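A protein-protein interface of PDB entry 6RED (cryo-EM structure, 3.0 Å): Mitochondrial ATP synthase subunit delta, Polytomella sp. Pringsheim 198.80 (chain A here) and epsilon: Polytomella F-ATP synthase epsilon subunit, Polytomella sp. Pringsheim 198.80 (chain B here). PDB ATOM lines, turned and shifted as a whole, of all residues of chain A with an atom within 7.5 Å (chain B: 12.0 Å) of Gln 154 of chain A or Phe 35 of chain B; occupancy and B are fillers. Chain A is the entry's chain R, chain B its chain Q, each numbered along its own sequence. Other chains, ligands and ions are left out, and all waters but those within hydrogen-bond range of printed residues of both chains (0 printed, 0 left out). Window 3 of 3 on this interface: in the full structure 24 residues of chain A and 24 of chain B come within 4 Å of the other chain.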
ATOM      1  N   PHE A 127      -2.637  33.442 -15.587  1.00  0.00           N
ATOM      2  CA  PHE A 127      -2.193  32.807 -16.818  1.00  0.00           C
ATOM      3  C   PHE A 127      -1.195  33.700 -17.531  1.00  0.00           C
ATOM      4  O   PHE A 127      -1.459  34.879 -17.759  1.00  0.00           O
ATOM      5  CB  PHE A 127      -3.369  32.529 -17.750  1.00  0.00           C
ATOM      6  CG  PHE A 127      -4.449  31.716 -17.133  1.00  0.00           C
ATOM      7  CD1 PHE A 127      -4.331  30.347 -17.046  1.00  0.00           C
ATOM      8  CD2 PHE A 127      -5.590  32.319 -16.640  1.00  0.00           C
ATOM      9  CE1 PHE A 127      -5.328  29.593 -16.478  1.00  0.00           C
ATOM     10  CE2 PHE A 127      -6.596  31.566 -16.075  1.00  0.00           C
ATOM     11  CZ  PHE A 127      -6.463  30.205 -15.993  1.00  0.00           C
ATOM     12  N   GLU A 148      -2.097  31.752 -27.128  1.00  0.00           N
ATOM     13  CA  GLU A 148      -1.597  30.685 -26.270  1.00  0.00           C
ATOM     14  C   GLU A 148      -1.396  31.241 -24.876  1.00  0.00           C
ATOM     15  O   GLU A 148      -0.613  32.173 -24.693  1.00  0.00           O
ATOM     16  CB  GLU A 148      -0.290  30.111 -26.801  1.00  0.00           C
ATOM     17  CG  GLU A 148       0.421  29.213 -25.818  1.00  0.00           C
ATOM     18  CD  GLU A 148      -0.248  27.875 -25.661  1.00  0.00           C
ATOM     19  OE1 GLU A 148      -0.689  27.308 -26.679  1.00  0.00           O
ATOM     20  OE2 GLU A 148      -0.341  27.388 -24.517  1.00  0.00           O
ATOM     21  N   ALA A 149      -2.089  30.670 -23.907  1.00  0.00           N
ATOM     22  CA  ALA A 149      -1.995  31.094 -22.517  1.00  0.00           C
ATOM     23  C   ALA A 149      -1.707  29.869 -21.664  1.00  0.00           C
ATOM     24  O   ALA A 149      -2.572  29.009 -21.488  1.00  0.00           O
ATOM     25  CB  ALA A 149      -3.269  31.779 -22.069  1.00  0.00           C
ATOM     26  N   ALA A 150      -0.492  29.791 -21.141  1.00  0.00           N
ATOM     27  CA  ALA A 150      -0.082  28.719 -20.251  1.00  0.00           C
ATOM     28  C   ALA A 150       0.111  29.293 -18.862  1.00  0.00           C
ATOM     29  O   ALA A 150       0.790  30.309 -18.704  1.00  0.00           O
ATOM     30  CB  ALA A 150       1.211  28.071 -20.731  1.00  0.00           C
ATOM     31  N   THR A 151      -0.486  28.649 -17.862  1.00  0.00           N
ATOM     32  CA  THR A 151      -0.343  29.123 -16.496  1.00  0.00           C
ATOM     33  C   THR A 151       1.079  28.891 -16.003  1.00  0.00           C
ATOM     34  O   THR A 151       1.847  28.111 -16.570  1.00  0.00           O
ATOM     35  CB  THR A 151      -1.351  28.445 -15.571  1.00  0.00           C
ATOM     36  OG1 THR A 151      -1.246  29.018 -14.265  1.00  0.00           O
ATOM     37  CG2 THR A 151      -1.093  26.975 -15.474  1.00  0.00           C
ATOM     38  N   LEU A 152       1.435  29.603 -14.931  1.00  0.00           N
ATOM     39  CA  LEU A 152       2.825  29.667 -14.501  1.00  0.00           C
ATOM     40  C   LEU A 152       3.332  28.359 -13.911  1.00  0.00           C
ATOM     41  O   LEU A 152       4.549  28.166 -13.837  1.00  0.00           O
ATOM     42  CB  LEU A 152       2.995  30.801 -13.495  1.00  0.00           C
ATOM     43  CG  LEU A 152       2.817  32.176 -14.142  1.00  0.00           C
ATOM     44  CD1 LEU A 152       2.606  33.259 -13.097  1.00  0.00           C
ATOM     45  CD2 LEU A 152       4.010  32.490 -15.022  1.00  0.00           C
ATOM     46  N   ASP A 153       2.437  27.457 -13.514  1.00  0.00           N
ATOM     47  CA  ASP A 153       2.837  26.132 -13.076  1.00  0.00           C
ATOM     48  C   ASP A 153       3.369  25.283 -14.217  1.00  0.00           C
ATOM     49  O   ASP A 153       4.224  24.424 -13.986  1.00  0.00           O
ATOM     50  CB  ASP A 153       1.649  25.416 -12.444  1.00  0.00           C
ATOM     51  CG  ASP A 153       1.111  26.145 -11.240  1.00  0.00           C
ATOM     52  OD1 ASP A 153       1.888  26.882 -10.597  1.00  0.00           O
ATOM     53  OD2 ASP A 153      -0.088  25.983 -10.930  1.00  0.00           O
ATOM     54  N   GLN A 154       2.893  25.514 -15.438  1.00  0.00           N
ATOM     55  CA  GLN A 154       3.197  24.669 -16.583  1.00  0.00           C
ATOM     56  C   GLN A 154       4.515  25.009 -17.248  1.00  0.00           C
ATOM     57  O   GLN A 154       4.944  24.272 -18.135  1.00  0.00           O
ATOM     58  CB  GLN A 154       2.079  24.771 -17.616  1.00  0.00           C
ATOM     59  CG  GLN A 154       0.748  24.264 -17.125  1.00  0.00           C
ATOM     60  CD  GLN A 154      -0.382  24.578 -18.076  1.00  0.00           C
ATOM     61  OE1 GLN A 154      -1.538  24.262 -17.806  1.00  0.00           O
ATOM     62  NE2 GLN A 154      -0.055  25.208 -19.194  1.00  0.00           N
ATOM     63  N   VAL A 155       5.165  26.098 -16.852  1.00  0.00           N
ATOM     64  CA  VAL A 155       6.402  26.551 -17.472  1.00  0.00           C
ATOM     65  C   VAL A 155       7.554  26.157 -16.562  1.00  0.00           C
ATOM     66  O   VAL A 155       7.480  26.356 -15.343  1.00  0.00           O
ATOM     67  CB  VAL A 155       6.382  28.072 -17.706  1.00  0.00           C
ATOM     68  CG1 VAL A 155       7.611  28.517 -18.459  1.00  0.00           C
ATOM     69  CG2 VAL A 155       5.135  28.474 -18.450  1.00  0.00           C
ATOM     70  N   ASP A 156       8.606  25.574 -17.145  1.00  0.00           N
ATOM     71  CA  ASP A 156       9.726  25.388 -16.233  1.00  0.00           C
ATOM     72  C   ASP A 156      10.761  26.483 -16.454  1.00  0.00           C
ATOM     73  O   ASP A 156      11.012  26.879 -17.597  1.00  0.00           O
ATOM     74  CB  ASP A 156      10.383  24.017 -16.414  1.00  0.00           C
ATOM     75  CG  ASP A 156      10.835  23.760 -17.835  1.00  0.00           C
ATOM     76  OD1 ASP A 156      10.259  24.365 -18.756  1.00  0.00           O
ATOM     77  OD2 ASP A 156      11.769  22.956 -18.031  1.00  0.00           O
ATOM     78  N   PRO A 157      11.362  27.021 -15.388  1.00  0.00           N
ATOM     79  CA  PRO A 157      12.275  28.156 -15.560  1.00  0.00           C
ATOM     80  C   PRO A 157      13.636  27.786 -16.118  1.00  0.00           C
ATOM     81  O   PRO A 157      14.349  28.679 -16.593  1.00  0.00           O
ATOM     82  CB  PRO A 157      12.398  28.722 -14.141  1.00  0.00           C
ATOM     83  CG  PRO A 157      12.108  27.580 -13.259  1.00  0.00           C
ATOM     84  CD  PRO A 157      11.125  26.707 -13.971  1.00  0.00           C
ATOM     85  N   ALA B  24       3.374  32.591 -29.833  1.00  0.00           N
ATOM     86  CA  ALA B  24       2.686  31.463 -29.214  1.00  0.00           C
ATOM     87  C   ALA B  24       3.537  30.207 -29.260  1.00  0.00           C
ATOM     88  O   ALA B  24       3.568  29.438 -28.293  1.00  0.00           O
ATOM     89  CB  ALA B  24       1.349  31.233 -29.904  1.00  0.00           C
ATOM     90  N   ASP B  25       4.263  30.007 -30.362  1.00  0.00           N
ATOM     91  CA  ASP B  25       5.148  28.857 -30.492  1.00  0.00           C
ATOM     92  C   ASP B  25       6.298  28.932 -29.507  1.00  0.00           C
ATOM     93  O   ASP B  25       6.625  27.940 -28.853  1.00  0.00           O
ATOM     94  CB  ASP B  25       5.692  28.773 -31.913  1.00  0.00           C
ATOM     95  CG  ASP B  25       4.655  28.320 -32.903  1.00  0.00           C
ATOM     96  OD1 ASP B  25       4.851  28.567 -34.111  1.00  0.00           O
ATOM     97  OD2 ASP B  25       3.634  27.747 -32.476  1.00  0.00           O
ATOM     98  N   LEU B  26       6.912  30.108 -29.378  1.00  0.00           N
ATOM     99  CA  LEU B  26       8.015  30.271 -28.444  1.00  0.00           C
ATOM    100  C   LEU B  26       7.563  30.240 -26.997  1.00  0.00           C
ATOM    101  O   LEU B  26       8.379  29.957 -26.121  1.00  0.00           O
ATOM    102  CB  LEU B  26       8.759  31.571 -28.722  1.00  0.00           C
ATOM    103  CG  LEU B  26       9.347  31.669 -30.123  1.00  0.00           C
ATOM    104  CD1 LEU B  26      10.097  32.963 -30.286  1.00  0.00           C
ATOM    105  CD2 LEU B  26      10.228  30.475 -30.443  1.00  0.00           C
ATOM    106  N   LEU B  27       6.299  30.527 -26.718  1.00  0.00           N
ATOM    107  CA  LEU B  27       5.801  30.227 -25.386  1.00  0.00           C
ATOM    108  C   LEU B  27       5.624  28.730 -25.200  1.00  0.00           C
ATOM    109  O   LEU B  27       5.904  28.205 -24.121  1.00  0.00           O
ATOM    110  CB  LEU B  27       4.480  30.952 -25.126  1.00  0.00           C
ATOM    111  CG  LEU B  27       3.735  30.619 -23.836  1.00  0.00           C
ATOM    112  CD1 LEU B  27       4.610  30.846 -22.630  1.00  0.00           C
ATOM    113  CD2 LEU B  27       2.496  31.440 -23.723  1.00  0.00           C
ATOM    114  N   ARG B  28       5.175  28.026 -26.240  1.00  0.00           N
ATOM    115  CA  ARG B  28       4.898  26.601 -26.095  1.00  0.00           C
ATOM    116  C   ARG B  28       6.157  25.766 -25.895  1.00  0.00           C
ATOM    117  O   ARG B  28       6.071  24.683 -25.316  1.00  0.00           O
ATOM    118  CB  ARG B  28       4.138  26.081 -27.311  1.00  0.00           C
ATOM    119  CG  ARG B  28       2.665  26.440 -27.350  1.00  0.00           C
ATOM    120  CD  ARG B  28       1.987  25.741 -28.505  1.00  0.00           C
ATOM    121  NE  ARG B  28       0.857  26.493 -29.028  1.00  0.00           N
ATOM    122  CZ  ARG B  28       0.854  27.090 -30.211  1.00  0.00           C
ATOM    123  NH1 ARG B  28       1.921  27.018 -30.986  1.00  0.00           N
ATOM    124  NH2 ARG B  28      -0.214  27.755 -30.621  1.00  0.00           N
ATOM    125  N   ASN B  29       7.317  26.249 -26.339  1.00  0.00           N
ATOM    126  CA  ASN B  29       8.540  25.461 -26.265  1.00  0.00           C
ATOM    127  C   ASN B  29       9.087  25.344 -24.853  1.00  0.00           C
ATOM    128  O   ASN B  29       9.804  24.386 -24.559  1.00  0.00           O
ATOM    129  CB  ASN B  29       9.603  26.068 -27.168  1.00  0.00           C
ATOM    130  CG  ASN B  29       9.251  25.948 -28.619  1.00  0.00           C
ATOM    131  OD1 ASN B  29       8.183  25.455 -28.959  1.00  0.00           O
ATOM    132  ND2 ASN B  29      10.146  26.388 -29.488  1.00  0.00           N
ATOM    133  N   VAL B  30       8.771  26.284 -23.977  1.00  0.00           N
ATOM    134  CA  VAL B  30       9.371  26.328 -22.658  1.00  0.00           C
ATOM    135  C   VAL B  30       8.435  25.765 -21.592  1.00  0.00           C
ATOM    136  O   VAL B  30       8.620  26.027 -20.405  1.00  0.00           O
ATOM    137  CB  VAL B  30       9.833  27.746 -22.304  1.00  0.00           C
ATOM    138  CG1 VAL B  30      10.865  28.198 -23.293  1.00  0.00           C
ATOM    139  CG2 VAL B  30       8.669  28.688 -22.321  1.00  0.00           C
ATOM    140  N   LEU B  31       7.440  24.987 -21.988  1.00  0.00           N
ATOM    141  CA  LEU B  31       6.584  24.396 -20.979  1.00  0.00           C
ATOM    142  C   LEU B  31       7.218  23.115 -20.450  1.00  0.00           C
ATOM    143  O   LEU B  31       8.190  22.596 -21.005  1.00  0.00           O
ATOM    144  CB  LEU B  31       5.193  24.117 -21.538  1.00  0.00           C
ATOM    145  CG  LEU B  31       4.490  25.209 -22.341  1.00  0.00           C
ATOM    146  CD1 LEU B  31       3.068  24.803 -22.643  1.00  0.00           C
ATOM    147  CD2 LEU B  31       4.497  26.516 -21.593  1.00  0.00           C
ATOM    148  N   LYS B  32       6.670  22.611 -19.351  1.00  0.00           N
ATOM    149  CA  LYS B  32       7.107  21.323 -18.840  1.00  0.00           C
ATOM    150  C   LYS B  32       6.591  20.211 -19.738  1.00  0.00           C
ATOM    151  O   LYS B  32       5.589  20.367 -20.437  1.00  0.00           O
ATOM    152  CB  LYS B  32       6.614  21.107 -17.416  1.00  0.00           C
ATOM    153  CG  LYS B  32       7.368  21.900 -16.385  1.00  0.00           C
ATOM    154  CD  LYS B  32       6.907  21.552 -14.992  1.00  0.00           C
ATOM    155  CE  LYS B  32       7.229  22.668 -14.030  1.00  0.00           C
ATOM    156  NZ  LYS B  32       6.543  23.919 -14.439  1.00  0.00           N
ATOM    157  N   GLU B  33       7.283  19.072 -19.691  1.00  0.00           N
ATOM    158  CA  GLU B  33       7.044  18.005 -20.658  1.00  0.00           C
ATOM    159  C   GLU B  33       5.657  17.346 -20.625  1.00  0.00           C
ATOM    160  O   GLU B  33       5.172  16.997 -21.718  1.00  0.00           O
ATOM    161  CB  GLU B  33       8.148  16.948 -20.520  1.00  0.00           C
ATOM    162  CG  GLU B  33       8.386  16.167 -21.794  1.00  0.00           C
ATOM    163  CD  GLU B  33       8.669  17.064 -22.982  1.00  0.00           C
ATOM    164  OE1 GLU B  33       9.574  17.918 -22.884  1.00  0.00           O
ATOM    165  OE2 GLU B  33       7.982  16.916 -24.014  1.00  0.00           O
ATOM    166  N   PRO B  34       4.970  17.153 -19.483  1.00  0.00           N
ATOM    167  CA  PRO B  34       3.556  16.744 -19.569  1.00  0.00           C
ATOM    168  C   PRO B  34       2.657  17.769 -20.228  1.00  0.00           C
ATOM    169  O   PRO B  34       1.622  17.393 -20.788  1.00  0.00           O
ATOM    170  CB  PRO B  34       3.162  16.535 -18.104  1.00  0.00           C
ATOM    171  CG  PRO B  34       4.391  16.169 -17.454  1.00  0.00           C
ATOM    172  CD  PRO B  34       5.440  17.010 -18.091  1.00  0.00           C
ATOM    173  N   PHE B  35       3.021  19.049 -20.182  1.00  0.00           N
ATOM    174  CA  PHE B  35       2.268  20.088 -20.862  1.00  0.00           C
ATOM    175  C   PHE B  35       2.876  20.484 -22.193  1.00  0.00           C
ATOM    176  O   PHE B  35       2.160  21.008 -23.048  1.00  0.00           O
ATOM    177  CB  PHE B  35       2.149  21.320 -19.968  1.00  0.00           C
ATOM    178  CG  PHE B  35       1.355  21.077 -18.723  1.00  0.00           C
ATOM    179  CD1 PHE B  35      -0.028  21.106 -18.754  1.00  0.00           C
ATOM    180  CD2 PHE B  35       1.984  20.811 -17.524  1.00  0.00           C
ATOM    181  CE1 PHE B  35      -0.765  20.884 -17.614  1.00  0.00           C
ATOM    182  CE2 PHE B  35       1.247  20.587 -16.380  1.00  0.00           C
ATOM    183  CZ  PHE B  35      -0.128  20.623 -16.430  1.00  0.00           C
ATOM    184  N   LYS B  36       4.173  20.246 -22.391  1.00  0.00           N
ATOM    185  CA  LYS B  36       4.762  20.422 -23.712  1.00  0.00           C
ATOM    186  C   LYS B  36       4.382  19.286 -24.653  1.00  0.00           C
ATOM    187  O   LYS B  36       4.505  19.439 -25.869  1.00  0.00           O
ATOM    188  CB  LYS B  36       6.283  20.538 -23.597  1.00  0.00           C
ATOM    189  CG  LYS B  36       6.976  21.178 -24.778  1.00  0.00           C
ATOM    190  CD  LYS B  36       8.448  21.338 -24.515  1.00  0.00           C
ATOM    191  CE  LYS B  36       9.239  21.188 -25.791  1.00  0.00           C
ATOM    192  NZ  LYS B  36       8.532  21.781 -26.944  1.00  0.00           N
ATOM    193  N   ALA B  37       3.918  18.154 -24.122  1.00  0.00           N
ATOM    194  CA  ALA B  37       3.466  17.078 -24.995  1.00  0.00           C
ATOM    195  C   ALA B  37       2.187  17.447 -25.731  1.00  0.00           C
ATOM    196  O   ALA B  37       2.074  17.191 -26.934  1.00  0.00           O
ATOM    197  CB  ALA B  37       3.264  15.795 -24.191  1.00  0.00           C
ATOM    198  N   LYS B  38       1.233  18.065 -25.047  1.00  0.00           N
ATOM    199  CA  LYS B  38      -0.029  18.443 -25.666  1.00  0.00           C
ATOM    200  C   LYS B  38       0.093  19.714 -26.502  1.00  0.00           C
ATOM    201  O   LYS B  38      -0.733  19.944 -27.391  1.00  0.00           O
ATOM    202  CB  LYS B  38      -1.105  18.621 -24.584  1.00  0.00           C
ATOM    203  CG  LYS B  38      -2.538  18.621 -25.092  1.00  0.00           C
ATOM    204  CD  LYS B  38      -3.544  18.754 -23.966  1.00  0.00           C
ATOM    205  CE  LYS B  38      -4.965  18.765 -24.509  1.00  0.00           C
ATOM    206  NZ  LYS B  38      -5.989  18.947 -23.449  1.00  0.00           N
ATOM    207  N   ALA B  39       1.123  20.517 -26.278  1.00  0.00           N
ATOM    208  CA  ALA B  39       1.275  21.751 -27.027  1.00  0.00           C
ATOM    209  C   ALA B  39       1.924  21.536 -28.383  1.00  0.00           C
ATOM    210  O   ALA B  39       1.898  22.441 -29.221  1.00  0.00           O
ATOM    211  CB  ALA B  39       2.086  22.763 -26.220  1.00  0.00           C
ATOM    212  N   GLN B  40       2.521  20.372 -28.625  1.00  0.00           N
ATOM    213  CA  GLN B  40       3.011  20.079 -29.964  1.00  0.00           C
ATOM    214  C   GLN B  40       1.909  19.600 -30.892  1.00  0.00           C
ATOM    215  O   GLN B  40       2.125  19.555 -32.106  1.00  0.00           O
ATOM    216  CB  GLN B  40       4.122  19.030 -29.920  1.00  0.00           C
ATOM    217  CG  GLN B  40       5.285  19.367 -29.007  1.00  0.00           C
ATOM    218  CD  GLN B  40       5.680  20.831 -29.044  1.00  0.00           C
ATOM    219  OE1 GLN B  40       6.057  21.359 -30.090  1.00  0.00           O
ATOM    220  NE2 GLN B  40       5.597  21.496 -27.897  1.00  0.00           N
ATOM    221  N   ALA B  41       0.749  19.232 -30.346  1.00  0.00           N
ATOM    222  CA  ALA B  41      -0.376  18.828 -31.179  1.00  0.00           C
ATOM    223  C   ALA B  41      -0.951  20.019 -31.924  1.00  0.00           C
ATOM    224  O   ALA B  41      -1.171  19.957 -33.137  1.00  0.00           O
ATOM    225  CB  ALA B  41      -1.454  18.171 -30.319  1.00  0.00           C
ATOM    226  N   ARG B  42      -1.174  21.122 -31.218  1.00  0.00           N
ATOM    227  CA  ARG B  42      -1.724  22.340 -31.792  1.00  0.00           C
ATOM    228  C   ARG B  42      -0.667  23.221 -32.438  1.00  0.00           C
ATOM    229  O   ARG B  42      -0.929  24.398 -32.689  1.00  0.00           O
ATOM    230  CB  ARG B  42      -2.465  23.125 -30.714  1.00  0.00           C
ATOM    231  CG  ARG B  42      -1.584  23.543 -29.582  1.00  0.00           C
ATOM    232  CD  ARG B  42      -2.316  24.442 -28.640  1.00  0.00           C
ATOM    233  NE  ARG B  42      -3.053  23.682 -27.646  1.00  0.00           N
ATOM    234  CZ  ARG B  42      -2.669  23.543 -26.383  1.00  0.00           C
ATOM    235  NH1 ARG B  42      -3.405  22.833 -25.545  1.00  0.00           N
ATOM    236  NH2 ARG B  42      -1.556  24.114 -25.957  1.00  0.00           N
ATOM    237  N   GLN B  43       0.510  22.676 -32.727  1.00  0.00           N
ATOM    238  CA  GLN B  43       1.586  23.422 -33.346  1.00  0.00           C
ATOM    239  C   GLN B  43       1.906  22.957 -34.754  1.00  0.00           C
ATOM    240  O   GLN B  43       2.518  23.716 -35.512  1.00  0.00           O
ATOM    241  CB  GLN B  43       2.854  23.324 -32.483  1.00  0.00           C
ATOM    242  CG  GLN B  43       3.819  24.479 -32.644  1.00  0.00           C
ATOM    243  CD  GLN B  43       4.893  24.508 -31.586  1.00  0.00           C
ATOM    244  OE1 GLN B  43       4.604  24.559 -30.392  1.00  0.00           O
ATOM    245  NE2 GLN B  43       6.142  24.476 -32.018  1.00  0.00           N
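No residue of chain B comes within 4 Å of Ala 149 of chain A.
Of the printed residues of chain B, Ala 150 of chain A touches Leu 31.
No residue of chain B comes within 4 Å of Thr 151 of chain A.
Printed residues of chain B within 4 Å of Asp 153 of chain A: Lys 32.
Gln 154 of chain A touches just these residues of chain B: Leu 31, Lys 32 and Phe 35.
Of the printed residues of chain A, Ala 24 of chain B touches Glu 148.
Printed residues of chain A within 4 Å of Val 30 of chain B: Val 155 (3.3 Å) and Asp 156 (2.9 Å).
Phe 35 of chain B touches one residue of chain A.
The nearest residue of chain B that does not touch Gln 154 of chain A is Val 30 of chain B (4.7 Å).
Of the 20 printed residues of chain B, 8 touch a printed residue of chain A.
Hydrophobic or aromatic side chains of chain B within 4 Å of the printed part of chain A: Ala 24, Leu 27, Leu 31 and Phe 35.
Hydrophobic or aromatic side chains of chain A that line the printed part of chain B: Ala 150 and Val 155.
Among the printed residues, Asp or Glu carboxylates within 4 Å of a Lys or Arg side-chain nitrogen of the other chain: Glu 148 of chain A with Arg 28 of chain B (2.9 Å) and Glu 148 of chain A with Arg 42 of chain B (3.4 Å).
Ala 24 of chain B touches Glu 148 of chain A.
CD2 of Leu 27 of chain B touches O of Glu 148 of chain A (3.3 Å).
Ala 150 of chain A touches Leu 31 of chain B (CB to CD2, 3.7 Å).
Gln 154 of chain A touches Leu 31 of chain B (O to CA, 3.3 Å).
Gln 154 of chain A touches Phe 35 of chain B.
Val 30 of chain B touches Val 155 of chain A (O to CG1, 3.3 Å).
Val 155 of chain A touches Leu 31 of chain B (CG2 to CD2, 3.8 Å).
Leu 31 of chain B touches Asp 156 of chain A.
Asp 156 of chain A touches Lys 32 of chain B.
The side-chain amino group (NZ) of Lys 32 of chain B sits at hydrogen-bond distance from the backbone carbonyl oxygen (O) of Val 155 of chain A, at 2.8 Å.
The side-chain carboxylate of Glu 148 of chain A lies within salt-bridge range of the guanidinium group of Arg 42 of chain B, 3.4 Å away.
O of Val 30 of chain B sits at hydrogen-bond distance from N of Asp 156 of chain A (3.3 Å).
The backbone carbonyl oxygen of Asp 153 of chain A sits at hydrogen-bond distance from the side-chain amino group of Lys 32 of chain B, at 2.4 Å.
OE1 of Glu 148 of chain A lies within salt-bridge range of NE of Arg 28 of chain B (2.9 Å).
The backbone NH (N) of Lys 32 of chain B sits at hydrogen-bond distance from the backbone carbonyl oxygen (O) of Gln 154 of chain A, at 2.7 Å.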
